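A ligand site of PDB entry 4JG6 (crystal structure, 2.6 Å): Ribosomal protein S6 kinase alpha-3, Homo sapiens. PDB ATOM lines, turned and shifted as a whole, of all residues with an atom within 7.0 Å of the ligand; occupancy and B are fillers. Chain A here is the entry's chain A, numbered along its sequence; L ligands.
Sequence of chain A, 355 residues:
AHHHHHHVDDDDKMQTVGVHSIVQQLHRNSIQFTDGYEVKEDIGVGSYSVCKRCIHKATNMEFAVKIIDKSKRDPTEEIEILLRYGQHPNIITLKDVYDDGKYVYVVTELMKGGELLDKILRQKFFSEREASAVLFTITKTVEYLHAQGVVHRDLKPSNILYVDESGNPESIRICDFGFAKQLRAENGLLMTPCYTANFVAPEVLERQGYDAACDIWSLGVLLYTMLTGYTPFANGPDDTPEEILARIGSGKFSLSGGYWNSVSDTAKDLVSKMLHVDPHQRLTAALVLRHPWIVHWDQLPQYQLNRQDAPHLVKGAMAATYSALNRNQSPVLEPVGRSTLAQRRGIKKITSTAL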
ATOM      1  N   ILE A  43     -10.025   6.113   9.602  1.00  0.00           N
ATOM      2  CA  ILE A  43      -9.106   6.757  10.534  1.00  0.00           C
ATOM      3  C   ILE A  43      -8.043   7.556   9.785  1.00  0.00           C
ATOM      4  O   ILE A  43      -7.881   8.750  10.013  1.00  0.00           O
ATOM      5  CB  ILE A  43      -8.404   5.717  11.433  1.00  0.00           C
ATOM      6  CG1 ILE A  43      -7.617   4.723  10.573  1.00  0.00           C
ATOM      7  CG2 ILE A  43      -9.430   4.993  12.294  1.00  0.00           C
ATOM      8  CD1 ILE A  43      -6.894   3.665  11.386  1.00  0.00           C
ATOM      9  N   SER A  49      -5.014   7.529  -0.928  1.00  0.00           N
ATOM     10  CA  SER A  49      -5.168   6.370  -0.063  1.00  0.00           C
ATOM     11  C   SER A  49      -6.086   6.675   1.109  1.00  0.00           C
ATOM     12  O   SER A  49      -6.224   7.826   1.528  1.00  0.00           O
ATOM     13  CB  SER A  49      -3.794   5.915   0.460  1.00  0.00           C
ATOM     14  OG  SER A  49      -3.119   6.978   1.094  1.00  0.00           O
ATOM     15  N   VAL A  50      -6.732   5.631   1.630  1.00  0.00           N
ATOM     16  CA  VAL A  50      -7.681   5.780   2.730  1.00  0.00           C
ATOM     17  C   VAL A  50      -7.319   4.851   3.888  1.00  0.00           C
ATOM     18  O   VAL A  50      -6.996   3.688   3.680  1.00  0.00           O
ATOM     19  CB  VAL A  50      -9.122   5.489   2.276  1.00  0.00           C
ATOM     20  CG1 VAL A  50      -9.192   4.139   1.569  1.00  0.00           C
ATOM     21  CG2 VAL A  50     -10.086   5.529   3.461  1.00  0.00           C
ATOM     22  N   CYS A  51      -7.397   5.387   5.102  1.00  0.00           N
ATOM     23  CA  CYS A  51      -7.105   4.601   6.302  1.00  0.00           C
ATOM     24  C   CYS A  51      -8.394   4.191   6.980  1.00  0.00           C
ATOM     25  O   CYS A  51      -9.347   4.959   7.060  1.00  0.00           O
ATOM     26  CB  CYS A  51      -6.236   5.414   7.272  1.00  0.00           C
ATOM     27  SG  CYS A  51      -4.638   5.911   6.594  1.00  0.00           S
ATOM     28  N   LYS A  52      -8.425   2.957   7.484  1.00  0.00           N
ATOM     29  CA  LYS A  52      -9.576   2.448   8.204  1.00  0.00           C
ATOM     30  C   LYS A  52      -9.132   1.533   9.329  1.00  0.00           C
ATOM     31  O   LYS A  52      -8.102   0.858   9.217  1.00  0.00           O
ATOM     32  CB  LYS A  52     -10.497   1.684   7.253  1.00  0.00           C
ATOM     33  CG  LYS A  52     -11.138   2.539   6.174  1.00  0.00           C
ATOM     34  CD  LYS A  52     -12.045   1.722   5.279  1.00  0.00           C
ATOM     35  CE  LYS A  52     -12.785   2.599   4.287  1.00  0.00           C
ATOM     36  NZ  LYS A  52     -13.687   1.796   3.401  1.00  0.00           N
ATOM     37  N   PHE A  63      -6.331  -3.401  14.283  1.00  0.00           N
ATOM     38  CA  PHE A  63      -5.183  -2.784  13.627  1.00  0.00           C
ATOM     39  C   PHE A  63      -5.647  -1.646  12.725  1.00  0.00           C
ATOM     40  O   PHE A  63      -6.829  -1.310  12.695  1.00  0.00           O
ATOM     41  CB  PHE A  63      -4.427  -3.820  12.797  1.00  0.00           C
ATOM     42  CG  PHE A  63      -3.918  -4.987  13.592  1.00  0.00           C
ATOM     43  CD1 PHE A  63      -2.660  -4.953  14.156  1.00  0.00           C
ATOM     44  CD2 PHE A  63      -4.697  -6.121  13.754  1.00  0.00           C
ATOM     45  CE1 PHE A  63      -2.185  -6.025  14.883  1.00  0.00           C
ATOM     46  CE2 PHE A  63      -4.226  -7.202  14.485  1.00  0.00           C
ATOM     47  CZ  PHE A  63      -2.970  -7.154  15.050  1.00  0.00           C
ATOM     48  N   ALA A  64      -4.709  -1.059  11.991  1.00  0.00           N
ATOM     49  CA  ALA A  64      -5.036  -0.031  11.011  1.00  0.00           C
ATOM     50  C   ALA A  64      -4.650  -0.523   9.614  1.00  0.00           C
ATOM     51  O   ALA A  64      -3.592  -1.124   9.433  1.00  0.00           O
ATOM     52  CB  ALA A  64      -4.300   1.251  11.339  1.00  0.00           C
ATOM     53  N   VAL A  65      -5.516  -0.275   8.644  1.00  0.00           N
ATOM     54  CA  VAL A  65      -5.259  -0.709   7.279  1.00  0.00           C
ATOM     55  C   VAL A  65      -5.314   0.465   6.304  1.00  0.00           C
ATOM     56  O   VAL A  65      -6.336   1.132   6.167  1.00  0.00           O
ATOM     57  CB  VAL A  65      -6.269  -1.791   6.825  1.00  0.00           C
ATOM     58  CG1 VAL A  65      -7.699  -1.300   6.996  1.00  0.00           C
ATOM     59  CG2 VAL A  65      -6.002  -2.196   5.382  1.00  0.00           C
ATOM     60  N   LYS A  66      -4.188   0.715   5.632  1.00  0.00           N
ATOM     61  CA  LYS A  66      -4.121   1.758   4.622  1.00  0.00           C
ATOM     62  C   LYS A  66      -4.387   1.157   3.249  1.00  0.00           C
ATOM     63  O   LYS A  66      -3.589   0.365   2.746  1.00  0.00           O
ATOM     64  CB  LYS A  66      -2.752   2.432   4.639  1.00  0.00           C
ATOM     65  CG  LYS A  66      -2.606   3.573   3.633  1.00  0.00           C
ATOM     66  CD  LYS A  66      -1.213   4.184   3.672  1.00  0.00           C
ATOM     67  CE  LYS A  66      -1.083   5.328   2.680  1.00  0.00           C
ATOM     68  NZ  LYS A  66       0.265   5.955   2.705  1.00  0.00           N
ATOM     69  N   GLU A  78       7.091   2.709  -0.601  1.00  0.00           N
ATOM     70  CA  GLU A  78       6.621   2.847   0.768  1.00  0.00           C
ATOM     71  C   GLU A  78       6.727   1.526   1.530  1.00  0.00           C
ATOM     72  O   GLU A  78       7.305   1.471   2.613  1.00  0.00           O
ATOM     73  CB  GLU A  78       5.177   3.356   0.789  1.00  0.00           C
ATOM     74  CG  GLU A  78       4.593   3.527   2.179  1.00  0.00           C
ATOM     75  CD  GLU A  78       3.171   4.050   2.153  1.00  0.00           C
ATOM     76  OE1 GLU A  78       2.626   4.247   1.045  1.00  0.00           O
ATOM     77  OE2 GLU A  78       2.582   4.251   3.235  1.00  0.00           O
ATOM     78  N   ILE A  92       6.201   3.470  12.890  1.00  0.00           N
ATOM     79  CA  ILE A  92       4.995   2.669  12.787  1.00  0.00           C
ATOM     80  C   ILE A  92       5.351   1.296  12.225  1.00  0.00           C
ATOM     81  O   ILE A  92       6.025   1.188  11.195  1.00  0.00           O
ATOM     82  CB  ILE A  92       3.917   3.351  11.921  1.00  0.00           C
ATOM     83  CG1 ILE A  92       2.627   2.528  11.934  1.00  0.00           C
ATOM     84  CG2 ILE A  92       4.423   3.545  10.489  1.00  0.00           C
ATOM     85  CD1 ILE A  92       1.475   3.195  11.228  1.00  0.00           C
ATOM     86  N   VAL A 106      -2.174  -2.160   3.344  1.00  0.00           N
ATOM     87  CA  VAL A 106      -1.072  -2.122   4.290  1.00  0.00           C
ATOM     88  C   VAL A 106      -1.610  -2.120   5.713  1.00  0.00           C
ATOM     89  O   VAL A 106      -2.200  -1.137   6.169  1.00  0.00           O
ATOM     90  CB  VAL A 106      -0.192  -0.877   4.086  1.00  0.00           C
ATOM     91  CG1 VAL A 106       0.942  -0.846   5.098  1.00  0.00           C
ATOM     92  CG2 VAL A 106       0.352  -0.843   2.669  1.00  0.00           C
ATOM     93  N   THR A 108      -1.057  -2.033   9.636  1.00  0.00           N
ATOM     94  CA  THR A 108      -0.082  -1.600  10.622  1.00  0.00           C
ATOM     95  C   THR A 108      -0.709  -1.565  12.016  1.00  0.00           C
ATOM     96  O   THR A 108      -1.894  -1.848  12.178  1.00  0.00           O
ATOM     97  CB  THR A 108       0.444  -0.195  10.298  1.00  0.00           C
ATOM     98  OG1 THR A 108      -0.609   0.762  10.431  1.00  0.00           O
ATOM     99  CG2 THR A 108       1.016  -0.151   8.883  1.00  0.00           C
ATOM    100  N   GLU A 109       0.104  -1.221  13.005  1.00  0.00           N
ATOM    101  CA  GLU A 109      -0.386  -1.077  14.364  1.00  0.00           C
ATOM    102  C   GLU A 109      -1.267   0.164  14.477  1.00  0.00           C
ATOM    103  O   GLU A 109      -1.000   1.191  13.853  1.00  0.00           O
ATOM    104  CB  GLU A 109       0.779  -0.998  15.359  1.00  0.00           C
ATOM    105  CG  GLU A 109       1.814   0.065  15.025  1.00  0.00           C
ATOM    106  CD  GLU A 109       2.982   0.068  15.994  1.00  0.00           C
ATOM    107  OE1 GLU A 109       2.915  -0.674  16.990  1.00  0.00           O
ATOM    108  OE2 GLU A 109       3.947   0.806  15.751  1.00  0.00           O
ATOM    109  N   LEU A 110      -2.335   0.056  15.266  1.00  0.00           N
ATOM    110  CA  LEU A 110      -3.299   1.138  15.420  1.00  0.00           C
ATOM    111  C   LEU A 110      -2.878   2.076  16.543  1.00  0.00           C
ATOM    112  O   LEU A 110      -2.625   1.642  17.668  1.00  0.00           O
ATOM    113  CB  LEU A 110      -4.682   0.553  15.707  1.00  0.00           C
ATOM    114  CG  LEU A 110      -5.845   1.544  15.843  1.00  0.00           C
ATOM    115  CD1 LEU A 110      -6.007   2.347  14.565  1.00  0.00           C
ATOM    116  CD2 LEU A 110      -7.122   0.811  16.190  1.00  0.00           C
ATOM    117  N   MET A 111      -2.816   3.370  16.237  1.00  0.00           N
ATOM    118  CA  MET A 111      -2.412   4.359  17.226  1.00  0.00           C
ATOM    119  C   MET A 111      -3.600   4.720  18.113  1.00  0.00           C
ATOM    120  O   MET A 111      -4.603   5.245  17.643  1.00  0.00           O
ATOM    121  CB  MET A 111      -1.914   5.625  16.531  1.00  0.00           C
ATOM    122  CG  MET A 111      -0.735   5.402  15.592  1.00  0.00           C
ATOM    123  SD  MET A 111       0.754   4.846  16.420  1.00  0.00           S
ATOM    124  CE  MET A 111       0.526   3.062  16.374  1.00  0.00           C
ATOM    125  N   LYS A 112      -3.476   4.412  19.401  1.00  0.00           N
ATOM    126  CA  LYS A 112      -4.536   4.685  20.366  1.00  0.00           C
ATOM    127  C   LYS A 112      -4.287   5.928  21.212  1.00  0.00           C
ATOM    128  O   LYS A 112      -5.092   6.267  22.079  1.00  0.00           O
ATOM    129  CB  LYS A 112      -4.747   3.459  21.259  1.00  0.00           C
ATOM    130  CG  LYS A 112      -5.015   2.194  20.471  1.00  0.00           C
ATOM    131  CD  LYS A 112      -6.287   2.309  19.630  1.00  0.00           C
ATOM    132  CE  LYS A 112      -7.533   2.178  20.485  1.00  0.00           C
ATOM    133  NZ  LYS A 112      -7.633   0.824  21.097  1.00  0.00           N
ATOM    134  N   SER A 158       0.645  15.814  12.137  1.00  0.00           N
ATOM    135  CA  SER A 158      -0.468  14.874  12.051  1.00  0.00           C
ATOM    136  C   SER A 158       0.017  13.447  11.778  1.00  0.00           C
ATOM    137  O   SER A 158      -0.738  12.486  11.963  1.00  0.00           O
ATOM    138  CB  SER A 158      -1.452  15.309  10.963  1.00  0.00           C
ATOM    139  OG  SER A 158      -0.806  15.501   9.716  1.00  0.00           O
ATOM    140  N   ASN A 159       1.263  13.308  11.339  1.00  0.00           N
ATOM    141  CA  ASN A 159       1.833  11.986  11.066  1.00  0.00           C
ATOM    142  C   ASN A 159       2.655  11.423  12.223  1.00  0.00           C
ATOM    143  O   ASN A 159       3.153  10.303  12.153  1.00  0.00           O
ATOM    144  CB  ASN A 159       2.679  12.036   9.794  1.00  0.00           C
ATOM    145  CG  ASN A 159       1.852  12.248   8.549  1.00  0.00           C
ATOM    146  OD1 ASN A 159       0.698  11.817   8.475  1.00  0.00           O
ATOM    147  ND2 ASN A 159       2.425  12.917   7.560  1.00  0.00           N
ATOM    148  N   LEU A 161       2.274  10.232  15.942  1.00  0.00           N
ATOM    149  CA  LEU A 161       1.181   9.854  16.833  1.00  0.00           C
ATOM    150  C   LEU A 161       1.666   9.019  18.011  1.00  0.00           C
ATOM    151  O   LEU A 161       2.764   8.468  17.993  1.00  0.00           O
ATOM    152  CB  LEU A 161       0.129   9.071  16.053  1.00  0.00           C
ATOM    153  CG  LEU A 161      -0.228   9.654  14.678  1.00  0.00           C
ATOM    154  CD1 LEU A 161      -1.145   8.702  13.920  1.00  0.00           C
ATOM    155  CD2 LEU A 161      -0.865  11.020  14.822  1.00  0.00           C
ATOM    156  N   CYS A 175       4.538   7.965  11.250  1.00  0.00           N
ATOM    157  CA  CYS A 175       3.598   7.253  10.407  1.00  0.00           C
ATOM    158  C   CYS A 175       3.439   7.872   9.015  1.00  0.00           C
ATOM    159  O   CYS A 175       3.925   8.979   8.768  1.00  0.00           O
ATOM    160  CB  CYS A 175       2.234   7.197  11.096  1.00  0.00           C
ATOM    161  SG  CYS A 175       2.317   6.725  12.845  1.00  0.00           S
ATOM    162  N   ASP A 176       2.766   7.146   8.121  1.00  0.00           N
ATOM    163  CA  ASP A 176       2.462   7.633   6.784  1.00  0.00           C
ATOM    164  C   ASP A 176       3.710   7.989   5.984  1.00  0.00           C
ATOM    165  O   ASP A 176       4.024   9.162   5.767  1.00  0.00           O
ATOM    166  CB  ASP A 176       1.521   8.835   6.831  1.00  0.00           C
ATOM    167  CG  ASP A 176       0.888   9.131   5.490  1.00  0.00           C
ATOM    168  OD1 ASP A 176      -0.318   9.470   5.466  1.00  0.00           O
ATOM    169  OD2 ASP A 176       1.586   9.020   4.452  1.00  0.00           O
ATOM    170  N   PHE A 177       4.429   6.952   5.550  1.00  0.00           N
ATOM    171  CA  PHE A 177       5.643   7.109   4.762  1.00  0.00           C
ATOM    172  C   PHE A 177       5.327   7.177   3.268  1.00  0.00           C
ATOM    173  O   PHE A 177       6.235   7.108   2.430  1.00  0.00           O
ATOM    174  CB  PHE A 177       6.614   5.964   5.049  1.00  0.00           C
ATOM    175  CG  PHE A 177       7.284   6.074   6.378  1.00  0.00           C
ATOM    176  CD1 PHE A 177       8.606   6.485   6.463  1.00  0.00           C
ATOM    177  CD2 PHE A 177       6.602   5.784   7.541  1.00  0.00           C
ATOM    178  CE1 PHE A 177       9.236   6.591   7.694  1.00  0.00           C
ATOM    179  CE2 PHE A 177       7.222   5.887   8.781  1.00  0.00           C
ATOM    180  CZ  PHE A 177       8.537   6.292   8.846  1.00  0.00           C
ATOM    181  N   GLY A 178       4.048   7.294   2.931  1.00  0.00           N
ATOM    182  CA  GLY A 178       3.606   7.277   1.555  1.00  0.00           C
ATOM    183  C   GLY A 178       4.417   8.162   0.623  1.00  0.00           C
ATOM    184  O   GLY A 178       4.551   7.860  -0.558  1.00  0.00           O
HETATM  185  C1  LIG L   1      -2.885   7.810   7.485  1.00  0.00           C
HETATM  186  C2  LIG L   1      -2.896   9.029   8.338  1.00  0.00           C
HETATM  187  N1  LIG L   1      -2.904   9.964   8.999  1.00  0.00           N
HETATM  188  C3  LIG L   1      -1.529   7.190   7.522  1.00  0.00           C
HETATM  189  N2  LIG L   1      -1.036   6.486   6.374  1.00  0.00           N
HETATM  190  O1  LIG L   1      -0.844   7.265   8.530  1.00  0.00           O
HETATM  191  C4  LIG L   1      -3.894   6.823   7.993  1.00  0.00           C
HETATM  192  C5  LIG L   1      -3.515   5.886   9.083  1.00  0.00           C
HETATM  193  C6  LIG L   1      -2.917   4.656   8.780  1.00  0.00           C
HETATM  194  C7  LIG L   1      -2.566   3.772   9.798  1.00  0.00           C
HETATM  195  C8  LIG L   1      -2.806   4.134  11.112  1.00  0.00           C
HETATM  196  N3  LIG L   1      -2.569   3.476  12.315  1.00  0.00           N
HETATM  197  N4  LIG L   1      -2.977   4.212  13.318  1.00  0.00           N
HETATM  198  C9  LIG L   1      -3.495   5.379  12.853  1.00  0.00           C
HETATM  199  C10 LIG L   1      -3.405   5.364  11.415  1.00  0.00           C
HETATM  200  C11 LIG L   1      -3.751   6.227  10.407  1.00  0.00           C
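NZ of Lys 66 is in salt-bridge range of OE2 of Glu 78 (2.9 Å). The side-chain carboxylate (OD2) of Asp 176 lies within salt-bridge range of the side-chain amino group (NZ) of Lys 66, at 3.8 Å. The side-chain carboxylate (OD2) of Asp 176 lies close to the backbone NH (N) of Gly 178. N of Ile 43 lies within hydrogen-bond range of O of Cys 51 (2.9 Å). The backbone carbonyl oxygen (O) of Ala 64 is in hydrogen-bond range of the backbone NH (N) of Thr 108 (2.7 Å). The backbone NH of Lys 66 is in hydrogen-bond range of the backbone carbonyl oxygen of Val 106 (2.8 Å).
N2 of the ligand sits at hydrogen-bond distance from OD1 of Asp 176, at 3.2 Å. The side-chain sulfur (SG) of Cys 51 is bonded to a carbon (C4) of the ligand, 1.8 Å away. N of Met 111 is in hydrogen-bond range of N4 of the ligand, 3.0 Å away. O of Glu 109 sits at hydrogen-bond distance from N3 of the ligand (3.2 Å).
Residues that only touch the ligand: Ala 64 (3.0 Å), Lys 66 (3.6 Å), Thr 108 (3.6 Å), Leu 110 (3.7 Å) and Ile 43 (3.9 Å). Hydrophobic or aromatic side chains within 4 Å of the ligand: Ile 43, Ala 64, Leu 110 and Met 111. Of the 24 residues printed, 9 come within 4 Å of the ligand.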
